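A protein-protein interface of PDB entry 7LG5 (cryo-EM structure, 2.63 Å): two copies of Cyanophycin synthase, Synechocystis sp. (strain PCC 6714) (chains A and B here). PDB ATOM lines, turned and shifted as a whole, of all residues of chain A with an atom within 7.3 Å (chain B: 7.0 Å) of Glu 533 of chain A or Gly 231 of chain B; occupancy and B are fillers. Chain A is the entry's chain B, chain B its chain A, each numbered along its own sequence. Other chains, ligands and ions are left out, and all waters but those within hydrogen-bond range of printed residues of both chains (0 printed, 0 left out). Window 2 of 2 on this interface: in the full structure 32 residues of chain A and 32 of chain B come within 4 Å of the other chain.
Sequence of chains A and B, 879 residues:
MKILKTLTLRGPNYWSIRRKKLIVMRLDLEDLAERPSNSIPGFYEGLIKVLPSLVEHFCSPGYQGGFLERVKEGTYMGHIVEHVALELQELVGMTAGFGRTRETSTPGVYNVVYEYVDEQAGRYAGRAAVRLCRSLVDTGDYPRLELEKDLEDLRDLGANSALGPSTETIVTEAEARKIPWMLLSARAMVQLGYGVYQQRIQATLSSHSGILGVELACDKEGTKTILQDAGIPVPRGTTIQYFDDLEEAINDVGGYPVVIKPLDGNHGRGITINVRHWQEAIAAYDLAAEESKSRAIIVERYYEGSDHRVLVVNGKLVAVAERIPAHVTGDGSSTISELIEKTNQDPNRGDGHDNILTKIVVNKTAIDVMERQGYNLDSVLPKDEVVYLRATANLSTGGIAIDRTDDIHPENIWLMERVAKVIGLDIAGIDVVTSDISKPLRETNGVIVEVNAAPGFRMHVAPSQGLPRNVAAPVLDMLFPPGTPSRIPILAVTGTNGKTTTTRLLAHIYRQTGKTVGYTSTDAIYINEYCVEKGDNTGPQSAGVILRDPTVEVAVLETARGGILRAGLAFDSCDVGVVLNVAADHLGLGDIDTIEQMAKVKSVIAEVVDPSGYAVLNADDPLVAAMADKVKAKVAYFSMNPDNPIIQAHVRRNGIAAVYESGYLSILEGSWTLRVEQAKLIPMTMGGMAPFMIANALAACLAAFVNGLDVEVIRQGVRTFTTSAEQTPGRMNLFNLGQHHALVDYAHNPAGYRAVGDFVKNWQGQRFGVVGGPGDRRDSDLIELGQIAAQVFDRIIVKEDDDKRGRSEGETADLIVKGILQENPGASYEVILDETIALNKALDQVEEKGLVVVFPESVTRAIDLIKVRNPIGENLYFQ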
ATOM      1  N   SER A 521       7.090 -18.654 -19.351  1.00  0.00           N
ATOM      2  CA  SER A 521       6.895 -17.306 -19.844  1.00  0.00           C
ATOM      3  C   SER A 521       5.587 -17.170 -20.591  1.00  0.00           C
ATOM      4  O   SER A 521       4.835 -18.134 -20.750  1.00  0.00           O
ATOM      5  CB  SER A 521       7.997 -16.929 -20.811  1.00  0.00           C
ATOM      6  OG  SER A 521       7.849 -17.594 -22.047  1.00  0.00           O
ATOM      7  N   ASP A 523       5.443 -16.818 -23.702  1.00  0.00           N
ATOM      8  CA  ASP A 523       5.554 -17.401 -25.028  1.00  0.00           C
ATOM      9  C   ASP A 523       5.444 -18.933 -25.016  1.00  0.00           C
ATOM     10  O   ASP A 523       4.894 -19.515 -25.962  1.00  0.00           O
ATOM     11  CB  ASP A 523       6.903 -17.072 -25.651  1.00  0.00           C
ATOM     12  CG  ASP A 523       7.217 -15.580 -25.828  1.00  0.00           C
ATOM     13  OD1 ASP A 523       6.411 -14.799 -26.310  1.00  0.00           O
ATOM     14  OD2 ASP A 523       8.321 -15.246 -25.484  1.00  0.00           O
ATOM     15  N   ALA A 524       6.050 -19.581 -23.992  1.00  0.00           N
ATOM     16  CA  ALA A 524       6.152 -21.044 -23.886  1.00  0.00           C
ATOM     17  C   ALA A 524       6.690 -21.542 -22.528  1.00  0.00           C
ATOM     18  O   ALA A 524       7.161 -20.765 -21.694  1.00  0.00           O
ATOM     19  CB  ALA A 524       7.042 -21.563 -24.989  1.00  0.00           C
ATOM     20  N   ILE A 525       6.634 -22.868 -22.336  1.00  0.00           N
ATOM     21  CA  ILE A 525       7.275 -23.557 -21.210  1.00  0.00           C
ATOM     22  C   ILE A 525       8.475 -24.305 -21.746  1.00  0.00           C
ATOM     23  O   ILE A 525       8.319 -25.121 -22.654  1.00  0.00           O
ATOM     24  CB  ILE A 525       6.364 -24.588 -20.505  1.00  0.00           C
ATOM     25  CG1 ILE A 525       5.177 -23.916 -19.965  1.00  0.00           C
ATOM     26  CG2 ILE A 525       7.135 -25.320 -19.412  1.00  0.00           C
ATOM     27  CD1 ILE A 525       4.110 -24.827 -19.397  1.00  0.00           C
ATOM     28  N   TYR A 526       9.654 -24.050 -21.169  1.00  0.00           N
ATOM     29  CA  TYR A 526      10.901 -24.688 -21.592  1.00  0.00           C
ATOM     30  C   TYR A 526      11.672 -25.424 -20.533  1.00  0.00           C
ATOM     31  O   TYR A 526      11.682 -25.031 -19.368  1.00  0.00           O
ATOM     32  CB  TYR A 526      11.898 -23.673 -22.115  1.00  0.00           C
ATOM     33  CG  TYR A 526      11.574 -23.036 -23.327  1.00  0.00           C
ATOM     34  CD1 TYR A 526      10.840 -21.921 -23.328  1.00  0.00           C
ATOM     35  CD2 TYR A 526      12.047 -23.560 -24.476  1.00  0.00           C
ATOM     36  CE1 TYR A 526      10.570 -21.325 -24.484  1.00  0.00           C
ATOM     37  CE2 TYR A 526      11.771 -22.978 -25.639  1.00  0.00           C
ATOM     38  CZ  TYR A 526      11.028 -21.860 -25.650  1.00  0.00           C
ATOM     39  OH  TYR A 526      10.733 -21.243 -26.832  1.00  0.00           O
ATOM     40  N   TYR A 530      14.422 -26.980 -24.680  1.00  0.00           N
ATOM     41  CA  TYR A 530      13.431 -27.751 -25.403  1.00  0.00           C
ATOM     42  C   TYR A 530      12.084 -27.185 -25.056  1.00  0.00           C
ATOM     43  O   TYR A 530      11.796 -26.897 -23.897  1.00  0.00           O
ATOM     44  CB  TYR A 530      13.470 -29.210 -25.036  1.00  0.00           C
ATOM     45  CG  TYR A 530      14.691 -29.900 -25.428  1.00  0.00           C
ATOM     46  CD1 TYR A 530      14.873 -30.286 -26.714  1.00  0.00           C
ATOM     47  CD2 TYR A 530      15.627 -30.183 -24.489  1.00  0.00           C
ATOM     48  CE1 TYR A 530      16.003 -30.948 -27.072  1.00  0.00           C
ATOM     49  CE2 TYR A 530      16.748 -30.849 -24.842  1.00  0.00           C
ATOM     50  CZ  TYR A 530      16.936 -31.231 -26.135  1.00  0.00           C
ATOM     51  OH  TYR A 530      18.069 -31.898 -26.488  1.00  0.00           O
ATOM     52  N   CYS A 531      11.219 -27.050 -26.025  1.00  0.00           N
ATOM     53  CA  CYS A 531       9.916 -26.496 -25.726  1.00  0.00           C
ATOM     54  C   CYS A 531       8.937 -27.591 -25.356  1.00  0.00           C
ATOM     55  O   CYS A 531       8.756 -28.548 -26.101  1.00  0.00           O
ATOM     56  CB  CYS A 531       9.404 -25.710 -26.911  1.00  0.00           C
ATOM     57  SG  CYS A 531       7.878 -24.933 -26.611  1.00  0.00           S
ATOM     58  N   VAL A 532       8.324 -27.455 -24.191  1.00  0.00           N
ATOM     59  CA  VAL A 532       7.374 -28.423 -23.680  1.00  0.00           C
ATOM     60  C   VAL A 532       5.968 -28.048 -24.155  1.00  0.00           C
ATOM     61  O   VAL A 532       5.233 -28.898 -24.648  1.00  0.00           O
ATOM     62  CB  VAL A 532       7.473 -28.468 -22.135  1.00  0.00           C
ATOM     63  CG1 VAL A 532       6.455 -29.384 -21.538  1.00  0.00           C
ATOM     64  CG2 VAL A 532       8.855 -28.917 -21.740  1.00  0.00           C
ATOM     65  N   GLU A 533       5.597 -26.780 -23.977  1.00  0.00           N
ATOM     66  CA  GLU A 533       4.283 -26.266 -24.401  1.00  0.00           C
ATOM     67  C   GLU A 533       4.416 -24.864 -24.972  1.00  0.00           C
ATOM     68  O   GLU A 533       5.277 -24.112 -24.536  1.00  0.00           O
ATOM     69  CB  GLU A 533       3.251 -26.236 -23.261  1.00  0.00           C
ATOM     70  CG  GLU A 533       2.918 -27.589 -22.665  1.00  0.00           C
ATOM     71  CD  GLU A 533       1.804 -27.610 -21.653  1.00  0.00           C
ATOM     72  OE1 GLU A 533       1.214 -26.594 -21.412  1.00  0.00           O
ATOM     73  OE2 GLU A 533       1.546 -28.668 -21.128  1.00  0.00           O
ATOM     74  N   LYS A 534       3.539 -24.472 -25.898  1.00  0.00           N
ATOM     75  CA  LYS A 534       3.541 -23.096 -26.427  1.00  0.00           C
ATOM     76  C   LYS A 534       2.294 -22.316 -26.043  1.00  0.00           C
ATOM     77  O   LYS A 534       1.251 -22.907 -25.774  1.00  0.00           O
ATOM     78  CB  LYS A 534       3.702 -23.084 -27.929  1.00  0.00           C
ATOM     79  CG  LYS A 534       5.022 -23.583 -28.380  1.00  0.00           C
ATOM     80  CD  LYS A 534       5.193 -23.444 -29.862  1.00  0.00           C
ATOM     81  CE  LYS A 534       6.562 -23.939 -30.302  1.00  0.00           C
ATOM     82  NZ  LYS A 534       6.755 -23.805 -31.772  1.00  0.00           N
ATOM     83  N   GLY A 535       2.395 -20.983 -26.038  1.00  0.00           N
ATOM     84  CA  GLY A 535       1.269 -20.112 -25.717  1.00  0.00           C
ATOM     85  C   GLY A 535       1.510 -19.390 -24.403  1.00  0.00           C
ATOM     86  O   GLY A 535       2.585 -19.492 -23.817  1.00  0.00           O
ATOM     87  N   ASP A 536       0.511 -18.659 -23.915  1.00  0.00           N
ATOM     88  CA  ASP A 536       0.723 -17.916 -22.685  1.00  0.00           C
ATOM     89  C   ASP A 536       0.700 -18.890 -21.564  1.00  0.00           C
ATOM     90  O   ASP A 536      -0.337 -19.473 -21.258  1.00  0.00           O
ATOM     91  CB  ASP A 536      -0.349 -16.849 -22.453  1.00  0.00           C
ATOM     92  CG  ASP A 536      -0.133 -16.001 -21.150  1.00  0.00           C
ATOM     93  OD1 ASP A 536       0.616 -16.419 -20.253  1.00  0.00           O
ATOM     94  OD2 ASP A 536      -0.707 -14.943 -21.075  1.00  0.00           O
ATOM     95  N   ASN A 537       1.864 -19.119 -20.997  1.00  0.00           N
ATOM     96  CA  ASN A 537       2.033 -20.098 -19.987  1.00  0.00           C
ATOM     97  C   ASN A 537       2.319 -19.521 -18.646  1.00  0.00           C
ATOM     98  O   ASN A 537       2.875 -20.212 -17.808  1.00  0.00           O
ATOM     99  CB  ASN A 537       3.024 -21.133 -20.426  1.00  0.00           C
ATOM    100  CG  ASN A 537       2.390 -22.084 -21.407  1.00  0.00           C
ATOM    101  OD1 ASN A 537       1.721 -23.009 -20.961  1.00  0.00           O
ATOM    102  ND2 ASN A 537       2.525 -21.893 -22.659  1.00  0.00           N
ATOM    103  N   GLN A 541      -1.029 -22.909 -13.202  1.00  0.00           N
ATOM    104  CA  GLN A 541      -1.154 -24.190 -13.851  1.00  0.00           C
ATOM    105  C   GLN A 541       0.128 -24.571 -14.564  1.00  0.00           C
ATOM    106  O   GLN A 541       0.407 -25.752 -14.736  1.00  0.00           O
ATOM    107  CB  GLN A 541      -2.321 -24.185 -14.820  1.00  0.00           C
ATOM    108  CG  GLN A 541      -3.684 -24.152 -14.156  1.00  0.00           C
ATOM    109  CD  GLN A 541      -4.082 -22.778 -13.602  1.00  0.00           C
ATOM    110  OE1 GLN A 541      -3.692 -21.716 -14.135  1.00  0.00           O
ATOM    111  NE2 GLN A 541      -4.856 -22.806 -12.517  1.00  0.00           N
ATOM    112  N   SER A 542       0.913 -23.580 -14.992  1.00  0.00           N
ATOM    113  CA  SER A 542       2.153 -23.857 -15.688  1.00  0.00           C
ATOM    114  C   SER A 542       3.268 -24.041 -14.710  1.00  0.00           C
ATOM    115  O   SER A 542       4.139 -24.895 -14.880  1.00  0.00           O
ATOM    116  CB  SER A 542       2.515 -22.714 -16.518  1.00  0.00           C
ATOM    117  OG  SER A 542       1.609 -22.497 -17.496  1.00  0.00           O
ATOM    118  N   VAL A 545       3.731 -27.516 -13.782  1.00  0.00           N
ATOM    119  CA  VAL A 545       4.300 -28.446 -14.738  1.00  0.00           C
ATOM    120  C   VAL A 545       5.774 -28.534 -14.448  1.00  0.00           C
ATOM    121  O   VAL A 545       6.343 -29.617 -14.438  1.00  0.00           O
ATOM    122  CB  VAL A 545       4.042 -28.012 -16.194  1.00  0.00           C
ATOM    123  CG1 VAL A 545       4.789 -28.903 -17.192  1.00  0.00           C
ATOM    124  CG2 VAL A 545       2.582 -28.087 -16.456  1.00  0.00           C
ATOM    125  N   ARG A 548       6.457 -30.237 -10.819  1.00  0.00           N
ATOM    126  CA  ARG A 548       6.256 -31.676 -10.776  1.00  0.00           C
ATOM    127  C   ARG A 548       7.237 -32.458 -11.653  1.00  0.00           C
ATOM    128  O   ARG A 548       7.206 -33.686 -11.655  1.00  0.00           O
ATOM    129  CB  ARG A 548       4.865 -32.067 -11.220  1.00  0.00           C
ATOM    130  CG  ARG A 548       3.726 -31.695 -10.306  1.00  0.00           C
ATOM    131  CD  ARG A 548       2.486 -32.381 -10.723  1.00  0.00           C
ATOM    132  NE  ARG A 548       2.073 -32.022 -12.081  1.00  0.00           N
ATOM    133  CZ  ARG A 548       1.265 -31.000 -12.433  1.00  0.00           C
ATOM    134  NH1 ARG A 548       0.742 -30.214 -11.518  1.00  0.00           N
ATOM    135  NH2 ARG A 548       0.998 -30.788 -13.713  1.00  0.00           N
ATOM    136  N   ILE B 226      -1.440 -39.130 -16.645  1.00  0.00           N
ATOM    137  CA  ILE B 226      -0.186 -38.642 -16.106  1.00  0.00           C
ATOM    138  C   ILE B 226       0.704 -38.052 -17.183  1.00  0.00           C
ATOM    139  O   ILE B 226       1.356 -37.040 -16.942  1.00  0.00           O
ATOM    140  CB  ILE B 226       0.554 -39.761 -15.320  1.00  0.00           C
ATOM    141  CG1 ILE B 226      -0.230 -40.177 -14.024  1.00  0.00           C
ATOM    142  CG2 ILE B 226       1.980 -39.387 -14.990  1.00  0.00           C
ATOM    143  CD1 ILE B 226      -0.417 -39.103 -12.943  1.00  0.00           C
ATOM    144  N   LEU B 227       0.792 -38.686 -18.347  1.00  0.00           N
ATOM    145  CA  LEU B 227       1.642 -38.143 -19.382  1.00  0.00           C
ATOM    146  C   LEU B 227       1.093 -36.889 -20.039  1.00  0.00           C
ATOM    147  O   LEU B 227       1.844 -35.938 -20.257  1.00  0.00           O
ATOM    148  CB  LEU B 227       1.894 -39.189 -20.467  1.00  0.00           C
ATOM    149  CG  LEU B 227       2.717 -40.422 -20.085  1.00  0.00           C
ATOM    150  CD1 LEU B 227       2.733 -41.350 -21.250  1.00  0.00           C
ATOM    151  CD2 LEU B 227       4.134 -40.054 -19.684  1.00  0.00           C
ATOM    152  N   GLN B 228      -0.211 -36.785 -20.274  1.00  0.00           N
ATOM    153  CA  GLN B 228      -0.654 -35.568 -20.938  1.00  0.00           C
ATOM    154  C   GLN B 228      -0.555 -34.361 -20.002  1.00  0.00           C
ATOM    155  O   GLN B 228      -0.305 -33.245 -20.451  1.00  0.00           O
ATOM    156  CB  GLN B 228      -2.037 -35.744 -21.558  1.00  0.00           C
ATOM    157  CG  GLN B 228      -3.170 -35.849 -20.640  1.00  0.00           C
ATOM    158  CD  GLN B 228      -4.438 -36.294 -21.368  1.00  0.00           C
ATOM    159  OE1 GLN B 228      -4.383 -37.045 -22.363  1.00  0.00           O
ATOM    160  NE2 GLN B 228      -5.580 -35.835 -20.883  1.00  0.00           N
ATOM    161  N   ASP B 229      -0.577 -34.590 -18.689  1.00  0.00           N
ATOM    162  CA  ASP B 229      -0.415 -33.519 -17.706  1.00  0.00           C
ATOM    163  C   ASP B 229       1.027 -33.003 -17.641  1.00  0.00           C
ATOM    164  O   ASP B 229       1.301 -31.997 -16.986  1.00  0.00           O
ATOM    165  CB  ASP B 229      -0.816 -33.969 -16.296  1.00  0.00           C
ATOM    166  CG  ASP B 229      -2.330 -34.131 -16.055  1.00  0.00           C
ATOM    167  OD1 ASP B 229      -3.111 -33.657 -16.851  1.00  0.00           O
ATOM    168  OD2 ASP B 229      -2.694 -34.698 -15.029  1.00  0.00           O
ATOM    169  N   ALA B 230       1.962 -33.734 -18.253  1.00  0.00           N
ATOM    170  CA  ALA B 230       3.373 -33.412 -18.288  1.00  0.00           C
ATOM    171  C   ALA B 230       3.768 -32.793 -19.625  1.00  0.00           C
ATOM    172  O   ALA B 230       4.957 -32.544 -19.867  1.00  0.00           O
ATOM    173  CB  ALA B 230       4.183 -34.668 -18.047  1.00  0.00           C
ATOM    174  N   GLY B 231       2.795 -32.594 -20.523  1.00  0.00           N
ATOM    175  CA  GLY B 231       3.088 -32.059 -21.841  1.00  0.00           C
ATOM    176  C   GLY B 231       3.630 -33.088 -22.843  1.00  0.00           C
ATOM    177  O   GLY B 231       4.339 -32.725 -23.776  1.00  0.00           O
ATOM    178  N   ILE B 232       3.338 -34.375 -22.652  1.00  0.00           N
ATOM    179  CA  ILE B 232       3.818 -35.439 -23.530  1.00  0.00           C
ATOM    180  C   ILE B 232       2.719 -35.851 -24.533  1.00  0.00           C
ATOM    181  O   ILE B 232       1.577 -36.022 -24.120  1.00  0.00           O
ATOM    182  CB  ILE B 232       4.295 -36.603 -22.648  1.00  0.00           C
ATOM    183  CG1 ILE B 232       5.501 -36.078 -21.792  1.00  0.00           C
ATOM    184  CG2 ILE B 232       4.603 -37.850 -23.449  1.00  0.00           C
ATOM    185  CD1 ILE B 232       5.965 -36.941 -20.671  1.00  0.00           C
ATOM    186  N   PRO B 233       2.980 -35.914 -25.870  1.00  0.00           N
ATOM    187  CA  PRO B 233       1.996 -36.276 -26.898  1.00  0.00           C
ATOM    188  C   PRO B 233       1.496 -37.720 -26.830  1.00  0.00           C
ATOM    189  O   PRO B 233       2.282 -38.661 -26.921  1.00  0.00           O
ATOM    190  CB  PRO B 233       2.783 -36.047 -28.190  1.00  0.00           C
ATOM    191  CG  PRO B 233       4.231 -36.169 -27.802  1.00  0.00           C
ATOM    192  CD  PRO B 233       4.321 -35.640 -26.396  1.00  0.00           C
ATOM    193  N   LEU B 415      12.895 -36.749 -25.014  1.00  0.00           N
ATOM    194  CA  LEU B 415      11.527 -37.032 -24.649  1.00  0.00           C
ATOM    195  C   LEU B 415      11.338 -38.438 -24.094  1.00  0.00           C
ATOM    196  O   LEU B 415      10.615 -38.604 -23.116  1.00  0.00           O
ATOM    197  CB  LEU B 415      10.615 -36.854 -25.855  1.00  0.00           C
ATOM    198  CG  LEU B 415       9.103 -37.129 -25.649  1.00  0.00           C
ATOM    199  CD1 LEU B 415       8.507 -36.203 -24.619  1.00  0.00           C
ATOM    200  CD2 LEU B 415       8.428 -36.973 -26.942  1.00  0.00           C
ATOM    201  N   ARG B 418      12.445 -38.688 -20.517  1.00  0.00           N
ATOM    202  CA  ARG B 418      11.528 -37.979 -19.638  1.00  0.00           C
ATOM    203  C   ARG B 418      10.279 -38.828 -19.370  1.00  0.00           C
ATOM    204  O   ARG B 418       9.803 -38.850 -18.241  1.00  0.00           O
ATOM    205  CB  ARG B 418      11.172 -36.595 -20.200  1.00  0.00           C
ATOM    206  CG  ARG B 418      10.498 -35.642 -19.181  1.00  0.00           C
ATOM    207  CD  ARG B 418      10.540 -34.176 -19.591  1.00  0.00           C
ATOM    208  NE  ARG B 418       9.602 -33.791 -20.633  1.00  0.00           N
ATOM    209  CZ  ARG B 418       8.316 -33.386 -20.412  1.00  0.00           C
ATOM    210  NH1 ARG B 418       7.817 -33.302 -19.210  1.00  0.00           N
ATOM    211  NH2 ARG B 418       7.522 -33.054 -21.405  1.00  0.00           N
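O of Ala 230 of chain B sits at hydrogen-bond distance from NH1 of Arg 418 of chain B (3.0 Å). The backbone carbonyl oxygen (O) of Ile 525 of chain A sits at hydrogen-bond distance from the backbone NH (N) of Val 532 of chain A. The backbone carbonyl oxygen (O) of Glu 533 of chain A sits at hydrogen-bond distance from the backbone NH (N) of Ile 525 of chain A (2.9 Å). The side-chain sulfur of Cys 531 of chain A sits at hydrogen-bond distance from the backbone carbonyl oxygen of Glu 533 of chain A (3.4 Å).
Hydrophobic or aromatic side chains of chain A within 4 Å of the printed part of chain B: Val 532. Along chain A the printed residues that touch a printed residue of chain B span positions 532 to 548. Among the printed residues, no Asp or Glu carboxylate lies within 4 Å of a Lys or Arg side-chain nitrogen of the other chain.
No position is printed for both chains. Of the 4 pairs that touch across the chains among the printed residues, none has its exchanged pair printed and touching as well.
Val 532 of chain A touches Ala 230 of chain B. Val 532 of chain A touches Arg 418 of chain B (CG1 to NH2, 3.8 Å). Gly 231 of chain B touches Glu 533 of chain A (CA to OE2, 3.8 Å). NH2 of Arg 548 of chain A touches O of Asp 229 of chain B, 3.5 Å away.
Of the printed residues of chain B, Val 532 of chain A touches Ala 230 (3.9 Å) and Arg 418 (3.8 Å). Glu 533 of chain A touches one residue of chain B. Gly 535 of chain A touches none of the printed residues of chain B. Ser 542 of chain A touches none of the printed residues of chain B. Of the printed residues of chain B, Arg 548 of chain A touches Asp 229. Printed residues of chain A within 4 Å of Asp 229 of chain B: Arg 548 (3.5 Å). Of the printed residues of chain A, Ala 230 of chain B touches Val 532 (3.9 Å). Gly 231 of chain B touches one residue of chain A. Printed residues of chain A within 4 Å of Arg 418 of chain B: Val 532.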
